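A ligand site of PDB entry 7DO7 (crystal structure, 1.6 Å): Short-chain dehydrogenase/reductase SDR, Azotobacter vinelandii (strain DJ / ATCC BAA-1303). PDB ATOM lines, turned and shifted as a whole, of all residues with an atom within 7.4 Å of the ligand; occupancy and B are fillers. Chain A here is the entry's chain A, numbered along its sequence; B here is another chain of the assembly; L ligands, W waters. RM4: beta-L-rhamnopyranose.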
ATOM      1  N   LEU A  13      18.199   0.122  37.508  1.00  0.00           N
ATOM      2  CA  LEU A  13      18.049   0.456  36.103  1.00  0.00           C
ATOM      3  C   LEU A  13      19.197   1.284  35.560  1.00  0.00           C
ATOM      4  O   LEU A  13      19.379   1.349  34.333  1.00  0.00           O
ATOM      5  CB  LEU A  13      16.721   1.198  35.892  1.00  0.00           C
ATOM      6  CG  LEU A  13      15.483   0.340  36.110  1.00  0.00           C
ATOM      7  CD1 LEU A  13      14.211   1.187  36.151  1.00  0.00           C
ATOM      8  CD2 LEU A  13      15.373  -0.733  35.033  1.00  0.00           C
ATOM      9  N   PHE A 242      13.065   6.333  33.900  1.00  0.00           N
ATOM     10  CA  PHE A 242      12.622   5.564  32.733  1.00  0.00           C
ATOM     11  C   PHE A 242      13.321   6.045  31.462  1.00  0.00           C
ATOM     12  O   PHE A 242      13.904   5.246  30.717  1.00  0.00           O
ATOM     13  CB  PHE A 242      11.097   5.708  32.601  1.00  0.00           C
ATOM     14  CG  PHE A 242      10.575   5.363  31.230  1.00  0.00           C
ATOM     15  CD1 PHE A 242      10.621   4.065  30.777  1.00  0.00           C
ATOM     16  CD2 PHE A 242      10.008   6.343  30.419  1.00  0.00           C
ATOM     17  CE1 PHE A 242      10.147   3.738  29.523  1.00  0.00           C
ATOM     18  CE2 PHE A 242       9.513   6.007  29.168  1.00  0.00           C
ATOM     19  CZ  PHE A 242       9.589   4.705  28.724  1.00  0.00           C
ATOM     20  N   SER A 245      16.896   5.085  31.076  1.00  0.00           N
ATOM     21  CA  SER A 245      17.151   3.658  31.185  1.00  0.00           C
ATOM     22  C   SER A 245      16.964   2.901  29.851  1.00  0.00           C
ATOM     23  O   SER A 245      16.439   3.418  28.856  1.00  0.00           O
ATOM     24  CB  SER A 245      16.251   3.064  32.262  1.00  0.00           C
ATOM     25  OG  SER A 245      14.934   2.889  31.773  1.00  0.00           O
ATOM     26  N   ASP A 246      17.400   1.639  29.865  1.00  0.00           N
ATOM     27  CA  ASP A 246      17.223   0.788  28.701  1.00  0.00           C
ATOM     28  C   ASP A 246      15.758   0.451  28.434  1.00  0.00           C
ATOM     29  O   ASP A 246      15.444  -0.062  27.354  1.00  0.00           O
ATOM     30  CB  ASP A 246      18.040  -0.495  28.849  1.00  0.00           C
ATOM     31  CG  ASP A 246      18.188  -1.259  27.519  1.00  0.00           C
ATOM     32  OD1 ASP A 246      18.565  -0.650  26.498  1.00  0.00           O
ATOM     33  OD2 ASP A 246      17.929  -2.488  27.500  1.00  0.00           O
ATOM     34  N   MET A 247      14.864   0.721  29.395  1.00  0.00           N
ATOM     35  CA  MET A 247      13.424   0.587  29.166  1.00  0.00           C
ATOM     36  C   MET A 247      12.959   1.501  28.051  1.00  0.00           C
ATOM     37  O   MET A 247      11.927   1.231  27.440  1.00  0.00           O
ATOM     38  CB  MET A 247      12.623   0.919  30.439  1.00  0.00           C
ATOM     39  CG  MET A 247      12.921   0.038  31.656  1.00  0.00           C
ATOM     40  SD  MET A 247      11.868   0.485  33.065  1.00  0.00           S
ATOM     41  CE  MET A 247      10.302  -0.095  32.461  1.00  0.00           C
ATOM     42  N   ALA A 248      13.714   2.547  27.772  1.00  0.00           N
ATOM     43  CA  ALA A 248      13.357   3.572  26.798  1.00  0.00           C
ATOM     44  C   ALA A 248      14.318   3.525  25.607  1.00  0.00           C
ATOM     45  O   ALA A 248      14.582   4.549  24.980  1.00  0.00           O
ATOM     46  CB  ALA A 248      13.358   4.954  27.454  1.00  0.00           C
ATOM     47  N   ARG A 249      14.823   2.318  25.290  1.00  0.00           N
ATOM     48  CA  ARG A 249      15.888   2.154  24.307  1.00  0.00           C
ATOM     49  C   ARG A 249      15.507   2.649  22.912  1.00  0.00           C
ATOM     50  O   ARG A 249      16.392   3.020  22.125  1.00  0.00           O
ATOM     51  CB  ARG A 249      16.292   0.677  24.243  1.00  0.00           C
ATOM     52  CG  ARG A 249      15.103  -0.254  24.071  1.00  0.00           C
ATOM     53  CD  ARG A 249      15.518  -1.653  23.610  1.00  0.00           C
ATOM     54  NE  ARG A 249      16.468  -2.268  24.531  1.00  0.00           N
ATOM     55  CZ  ARG A 249      16.768  -3.558  24.528  1.00  0.00           C
ATOM     56  NH1 ARG A 249      17.648  -4.035  25.400  1.00  0.00           N
ATOM     57  NH2 ARG A 249      16.176  -4.373  23.658  1.00  0.00           N
ATOM     58  N   TYR A 250      14.218   2.627  22.567  1.00  0.00           N
ATOM     59  CA  TYR A 250      13.777   3.102  21.257  1.00  0.00           C
ATOM     60  C   TYR A 250      13.033   4.430  21.349  1.00  0.00           C
ATOM     61  O   TYR A 250      12.337   4.818  20.400  1.00  0.00           O
ATOM     62  CB  TYR A 250      12.916   2.026  20.571  1.00  0.00           C
ATOM     63  CG  TYR A 250      12.816   2.140  19.057  1.00  0.00           C
ATOM     64  CD1 TYR A 250      13.948   2.122  18.249  1.00  0.00           C
ATOM     65  CD2 TYR A 250      11.580   2.236  18.429  1.00  0.00           C
ATOM     66  CE1 TYR A 250      13.847   2.218  16.846  1.00  0.00           C
ATOM     67  CE2 TYR A 250      11.464   2.324  17.061  1.00  0.00           C
ATOM     68  CZ  TYR A 250      12.611   2.319  16.257  1.00  0.00           C
ATOM     69  OH  TYR A 250      12.491   2.413  14.881  1.00  0.00           O
ATOM     70  N   LEU B  13       8.576  -4.778  38.884  1.00  0.00           N
ATOM     71  CA  LEU B  13       7.813  -3.538  38.782  1.00  0.00           C
ATOM     72  C   LEU B  13       6.309  -3.768  38.803  1.00  0.00           C
ATOM     73  O   LEU B  13       5.546  -2.826  39.079  1.00  0.00           O
ATOM     74  CB  LEU B  13       8.204  -2.789  37.495  1.00  0.00           C
ATOM     75  CG  LEU B  13       9.565  -2.103  37.446  1.00  0.00           C
ATOM     76  CD1 LEU B  13       9.778  -1.486  36.043  1.00  0.00           C
ATOM     77  CD2 LEU B  13       9.686  -1.037  38.507  1.00  0.00           C
ATOM     78  N   ALA B  31       5.262  -9.475  23.133  1.00  0.00           N
ATOM     79  CA  ALA B  31       6.431  -8.995  23.859  1.00  0.00           C
ATOM     80  C   ALA B  31       6.028  -8.267  25.132  1.00  0.00           C
ATOM     81  O   ALA B  31       6.719  -8.367  26.152  1.00  0.00           O
ATOM     82  CB  ALA B  31       7.263  -8.089  22.953  1.00  0.00           C
ATOM     83  N   ALA B  32       4.927  -7.520  25.078  1.00  0.00           N
ATOM     84  CA  ALA B  32       4.472  -6.800  26.266  1.00  0.00           C
ATOM     85  C   ALA B  32       3.985  -7.749  27.357  1.00  0.00           C
ATOM     86  O   ALA B  32       4.270  -7.543  28.549  1.00  0.00           O
ATOM     87  CB  ALA B  32       3.373  -5.816  25.879  1.00  0.00           C
ATOM     88  N   ARG B  34       4.874 -10.878  27.762  1.00  0.00           N
ATOM     89  CA  ARG B  34       6.051 -11.597  28.249  1.00  0.00           C
ATOM     90  C   ARG B  34       6.818 -10.768  29.288  1.00  0.00           C
ATOM     91  O   ARG B  34       7.174 -11.260  30.363  1.00  0.00           O
ATOM     92  CB  ARG B  34       6.955 -11.982  27.075  1.00  0.00           C
ATOM     93  CG  ARG B  34       8.079 -12.963  27.465  1.00  0.00           C
ATOM     94  CD  ARG B  34       9.199 -12.959  26.429  1.00  0.00           C
ATOM     95  NE  ARG B  34       8.716 -13.466  25.149  1.00  0.00           N
ATOM     96  CZ  ARG B  34       8.762 -12.789  24.007  1.00  0.00           C
ATOM     97  NH1 ARG B  34       9.241 -11.559  23.971  1.00  0.00           N
ATOM     98  NH2 ARG B  34       8.309 -13.350  22.892  1.00  0.00           N
ATOM     99  N   GLU B  35       7.063  -9.486  28.983  1.00  0.00           N
ATOM    100  CA  GLU B  35       7.841  -8.680  29.909  1.00  0.00           C
ATOM    101  C   GLU B  35       7.033  -8.328  31.141  1.00  0.00           C
ATOM    102  O   GLU B  35       7.593  -8.151  32.225  1.00  0.00           O
ATOM    103  CB  GLU B  35       8.354  -7.419  29.200  1.00  0.00           C
ATOM    104  CG  GLU B  35       9.144  -6.427  30.072  1.00  0.00           C
ATOM    105  CD  GLU B  35      10.455  -6.981  30.628  1.00  0.00           C
ATOM    106  OE1 GLU B  35      10.950  -8.016  30.129  1.00  0.00           O
ATOM    107  OE2 GLU B  35      10.994  -6.372  31.571  1.00  0.00           O
ATOM    108  N   ARG B  38       7.601 -11.241  33.303  1.00  0.00           N
ATOM    109  CA  ARG B  38       8.959 -11.119  33.820  1.00  0.00           C
ATOM    110  C   ARG B  38       9.034 -10.140  34.982  1.00  0.00           C
ATOM    111  O   ARG B  38       9.890 -10.290  35.866  1.00  0.00           O
ATOM    112  CB  ARG B  38       9.910 -10.650  32.719  1.00  0.00           C
ATOM    113  CG  ARG B  38      10.216 -11.684  31.655  1.00  0.00           C
ATOM    114  CD  ARG B  38      11.118 -12.763  32.224  1.00  0.00           C
ATOM    115  NE  ARG B  38      11.779 -13.544  31.184  1.00  0.00           N
ATOM    116  CZ  ARG B  38      12.779 -14.382  31.407  1.00  0.00           C
ATOM    117  NH1 ARG B  38      13.248 -14.546  32.641  1.00  0.00           N
ATOM    118  NH2 ARG B  38      13.327 -15.049  30.404  1.00  0.00           N
ATOM    119  N   GLN B  39       8.199  -9.110  34.981  1.00  0.00           N
ATOM    120  CA  GLN B  39       8.160  -8.124  36.035  1.00  0.00           C
ATOM    121  C   GLN B  39       7.235  -8.519  37.197  1.00  0.00           C
ATOM    122  O   GLN B  39       6.946  -7.683  38.053  1.00  0.00           O
ATOM    123  CB  GLN B  39       7.757  -6.762  35.472  1.00  0.00           C
ATOM    124  CG  GLN B  39       8.803  -6.187  34.532  1.00  0.00           C
ATOM    125  CD  GLN B  39      10.099  -5.830  35.248  1.00  0.00           C
ATOM    126  OE1 GLN B  39      10.086  -5.370  36.385  1.00  0.00           O
ATOM    127  NE2 GLN B  39      11.232  -6.041  34.572  1.00  0.00           N
ATOM    128  N   GLU B 232      11.481  -3.294  17.009  1.00  0.00           N
ATOM    129  CA  GLU B 232      11.071  -4.668  17.215  1.00  0.00           C
ATOM    130  C   GLU B 232      10.105  -4.702  18.388  1.00  0.00           C
ATOM    131  O   GLU B 232      10.054  -3.759  19.177  1.00  0.00           O
ATOM    132  CB  GLU B 232      12.287  -5.570  17.463  1.00  0.00           C
ATOM    133  CG  GLU B 232      12.970  -5.363  18.802  1.00  0.00           C
ATOM    134  CD  GLU B 232      13.993  -6.463  19.100  1.00  0.00           C
ATOM    135  OE1 GLU B 232      14.660  -6.395  20.154  1.00  0.00           O
ATOM    136  OE2 GLU B 232      14.155  -7.393  18.265  1.00  0.00           O
ATOM    137  N   PRO B 233       9.295  -5.757  18.502  1.00  0.00           N
ATOM    138  CA  PRO B 233       8.284  -5.792  19.591  1.00  0.00           C
ATOM    139  C   PRO B 233       8.840  -5.484  20.964  1.00  0.00           C
ATOM    140  O   PRO B 233       8.188  -4.753  21.732  1.00  0.00           O
ATOM    141  CB  PRO B 233       7.738  -7.211  19.487  1.00  0.00           C
ATOM    142  CG  PRO B 233       7.818  -7.520  18.010  1.00  0.00           C
ATOM    143  CD  PRO B 233       9.087  -6.859  17.528  1.00  0.00           C
ATOM    144  N   ASP B 234      10.029  -5.974  21.299  1.00  0.00           N
ATOM    145  CA  ASP B 234      10.581  -5.721  22.616  1.00  0.00           C
ATOM    146  C   ASP B 234      10.835  -4.236  22.864  1.00  0.00           C
ATOM    147  O   ASP B 234      10.946  -3.828  24.021  1.00  0.00           O
ATOM    148  CB  ASP B 234      11.882  -6.506  22.816  1.00  0.00           C
ATOM    149  CG  ASP B 234      11.638  -7.959  23.228  1.00  0.00           C
ATOM    150  OD1 ASP B 234      10.582  -8.248  23.816  1.00  0.00           O
ATOM    151  OD2 ASP B 234      12.528  -8.803  22.969  1.00  0.00           O
ATOM    152  N   ASP B 235      10.931  -3.425  21.800  1.00  0.00           N
ATOM    153  CA  ASP B 235      11.123  -1.991  21.989  1.00  0.00           C
ATOM    154  C   ASP B 235       9.936  -1.341  22.669  1.00  0.00           C
ATOM    155  O   ASP B 235      10.080  -0.264  23.255  1.00  0.00           O
ATOM    156  CB  ASP B 235      11.371  -1.310  20.647  1.00  0.00           C
ATOM    157  CG  ASP B 235      12.758  -1.586  20.114  1.00  0.00           C
ATOM    158  OD1 ASP B 235      13.688  -1.676  20.930  1.00  0.00           O
ATOM    159  OD2 ASP B 235      12.906  -1.738  18.874  1.00  0.00           O
ATOM    160  N   LEU B 236       8.744  -1.947  22.589  1.00  0.00           N
ATOM    161  CA  LEU B 236       7.588  -1.375  23.262  1.00  0.00           C
ATOM    162  C   LEU B 236       7.360  -1.955  24.649  1.00  0.00           C
ATOM    163  O   LEU B 236       6.525  -1.421  25.382  1.00  0.00           O
ATOM    164  CB  LEU B 236       6.320  -1.592  22.433  1.00  0.00           C
ATOM    165  CG  LEU B 236       5.975  -0.553  21.369  1.00  0.00           C
ATOM    166  CD1 LEU B 236       5.646   0.783  22.026  1.00  0.00           C
ATOM    167  CD2 LEU B 236       7.111  -0.392  20.361  1.00  0.00           C
ATOM    168  N   ALA B 237       8.068  -3.024  25.038  1.00  0.00           N
ATOM    169  CA  ALA B 237       7.765  -3.642  26.324  1.00  0.00           C
ATOM    170  C   ALA B 237       8.137  -2.735  27.494  1.00  0.00           C
ATOM    171  O   ALA B 237       7.363  -2.598  28.458  1.00  0.00           O
ATOM    172  CB  ALA B 237       8.480  -4.994  26.420  1.00  0.00           C
ATOM    173  N   GLY B 238       9.316  -2.126  27.457  1.00  0.00           N
ATOM    174  CA  GLY B 238       9.721  -1.196  28.482  1.00  0.00           C
ATOM    175  C   GLY B 238       8.773  -0.029  28.691  1.00  0.00           C
ATOM    176  O   GLY B 238       8.379   0.278  29.815  1.00  0.00           O
ATOM    177  N   PRO B 239       8.385   0.641  27.601  1.00  0.00           N
ATOM    178  CA  PRO B 239       7.461   1.777  27.776  1.00  0.00           C
ATOM    179  C   PRO B 239       6.088   1.383  28.309  1.00  0.00           C
ATOM    180  O   PRO B 239       5.495   2.139  29.080  1.00  0.00           O
ATOM    181  CB  PRO B 239       7.376   2.359  26.365  1.00  0.00           C
ATOM    182  CG  PRO B 239       8.678   1.999  25.720  1.00  0.00           C
ATOM    183  CD  PRO B 239       8.983   0.618  26.250  1.00  0.00           C
ATOM    184  N   VAL B 241       5.456  -1.344  30.272  1.00  0.00           N
ATOM    185  CA  VAL B 241       5.673  -1.666  31.692  1.00  0.00           C
ATOM    186  C   VAL B 241       5.793  -0.389  32.509  1.00  0.00           C
ATOM    187  O   VAL B 241       5.215  -0.259  33.588  1.00  0.00           O
ATOM    188  CB  VAL B 241       6.913  -2.573  31.868  1.00  0.00           C
ATOM    189  CG1 VAL B 241       7.311  -2.654  33.340  1.00  0.00           C
ATOM    190  CG2 VAL B 241       6.644  -3.974  31.346  1.00  0.00           C
ATOM    191  N   PHE B 242       6.580   0.582  32.012  1.00  0.00           N
ATOM    192  CA  PHE B 242       6.701   1.846  32.717  1.00  0.00           C
ATOM    193  C   PHE B 242       5.339   2.469  32.971  1.00  0.00           C
ATOM    194  O   PHE B 242       5.011   2.838  34.100  1.00  0.00           O
ATOM    195  CB  PHE B 242       7.585   2.814  31.923  1.00  0.00           C
ATOM    196  CG  PHE B 242       7.379   4.267  32.295  1.00  0.00           C
ATOM    197  CD1 PHE B 242       7.800   4.751  33.529  1.00  0.00           C
ATOM    198  CD2 PHE B 242       6.760   5.129  31.411  1.00  0.00           C
ATOM    199  CE1 PHE B 242       7.613   6.070  33.874  1.00  0.00           C
ATOM    200  CE2 PHE B 242       6.557   6.452  31.755  1.00  0.00           C
ATOM    201  CZ  PHE B 242       6.987   6.926  32.988  1.00  0.00           C
HETATM  202  C1  RM4 L   1      12.789  -3.977  29.271  1.00  0.00           C
HETATM  203  C2  RM4 L   1      14.257  -3.721  28.897  1.00  0.00           C
HETATM  204  C3  RM4 L   1      14.530  -3.658  27.394  1.00  0.00           C
HETATM  205  C4  RM4 L   1      13.880  -4.829  26.653  1.00  0.00           C
HETATM  206  C5  RM4 L   1      12.876  -5.572  27.545  1.00  0.00           C
HETATM  207  C6  RM4 L   1      11.967  -6.503  26.756  1.00  0.00           C
HETATM  208  O1  RM4 L   1      12.146  -2.764  29.673  1.00  0.00           O
HETATM  209  O2  RM4 L   1      14.693  -2.511  29.535  1.00  0.00           O
HETATM  210  O3  RM4 L   1      14.079  -2.408  26.825  1.00  0.00           O
HETATM  211  O4  RM4 L   1      14.912  -5.704  26.180  1.00  0.00           O
HETATM  212  O5  RM4 L   1      12.075  -4.594  28.196  1.00  0.00           O
HETATM  213  O   HOH W   1      10.690  -3.828  31.868  1.00  0.00           O
HETATM  214  O   HOH W   2      11.539  -1.918  25.644  1.00  0.00           O
HETATM  215  O   HOH W   3      14.200  -3.520  32.500  1.00  0.00           O
HETATM  216  O   HOH W   4      13.727  -6.135  31.611  1.00  0.00           O
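Glu 35 of chain B touches the ligand (CD to O5, 3.8 Å). Asp 234 of chain B touches the ligand. Ala 237 of chain B touches the ligand (CB to C6, 3.8 Å). CA of Gly 238 of chain B touches O1 of the ligand, 3.1 Å away. Hydrophobic or aromatic side chains that line the ligand: Met 247 and Ala 237 of chain B. Seven residues have an atom within 4 Å of the ligand: Asp 246, Met 247, Arg 249, Glu 35 of chain B, Asp 234 of chain B, Ala 237 of chain B and Gly 238 of chain B. The nearest printed residue that does not touch the ligand is Ala 248 (5.1 Å).
The guanidinium group (NH1) of Arg 249 lies within salt-bridge range of the side-chain carboxylate (OD2) of Asp 246 (2.6 Å). The side-chain carboxylate (OE2) of Glu 35 of chain B sits at hydrogen-bond distance from the side-chain amide nitrogen (NE2) of Gln 39 of chain B (3.0 Å). The backbone NH of Met 247 lies close to the side-chain hydroxyl of Ser 245 (3.2 Å).
Water W1 lies within hydrogen-bond range of the side-chain carboxylate (OE2) of Glu 35 of chain B and an oxygen (O1) of the ligand. Water W2 lies within hydrogen-bond range of O of Asp 234 of chain B, O3 of the ligand, N of Gly 238 of chain B and O of Asp 235 of chain B.
O of Asp 246 sits at hydrogen-bond distance from O3 of the ligand, at 2.8 Å. The backbone NH (N) of Met 247 is in hydrogen-bond range of an oxygen (O2) of the ligand, 3.2 Å away. The guanidinium group of Arg 249 lies within hydrogen-bond range of an oxygen (O4) of the ligand (3.1 Å).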
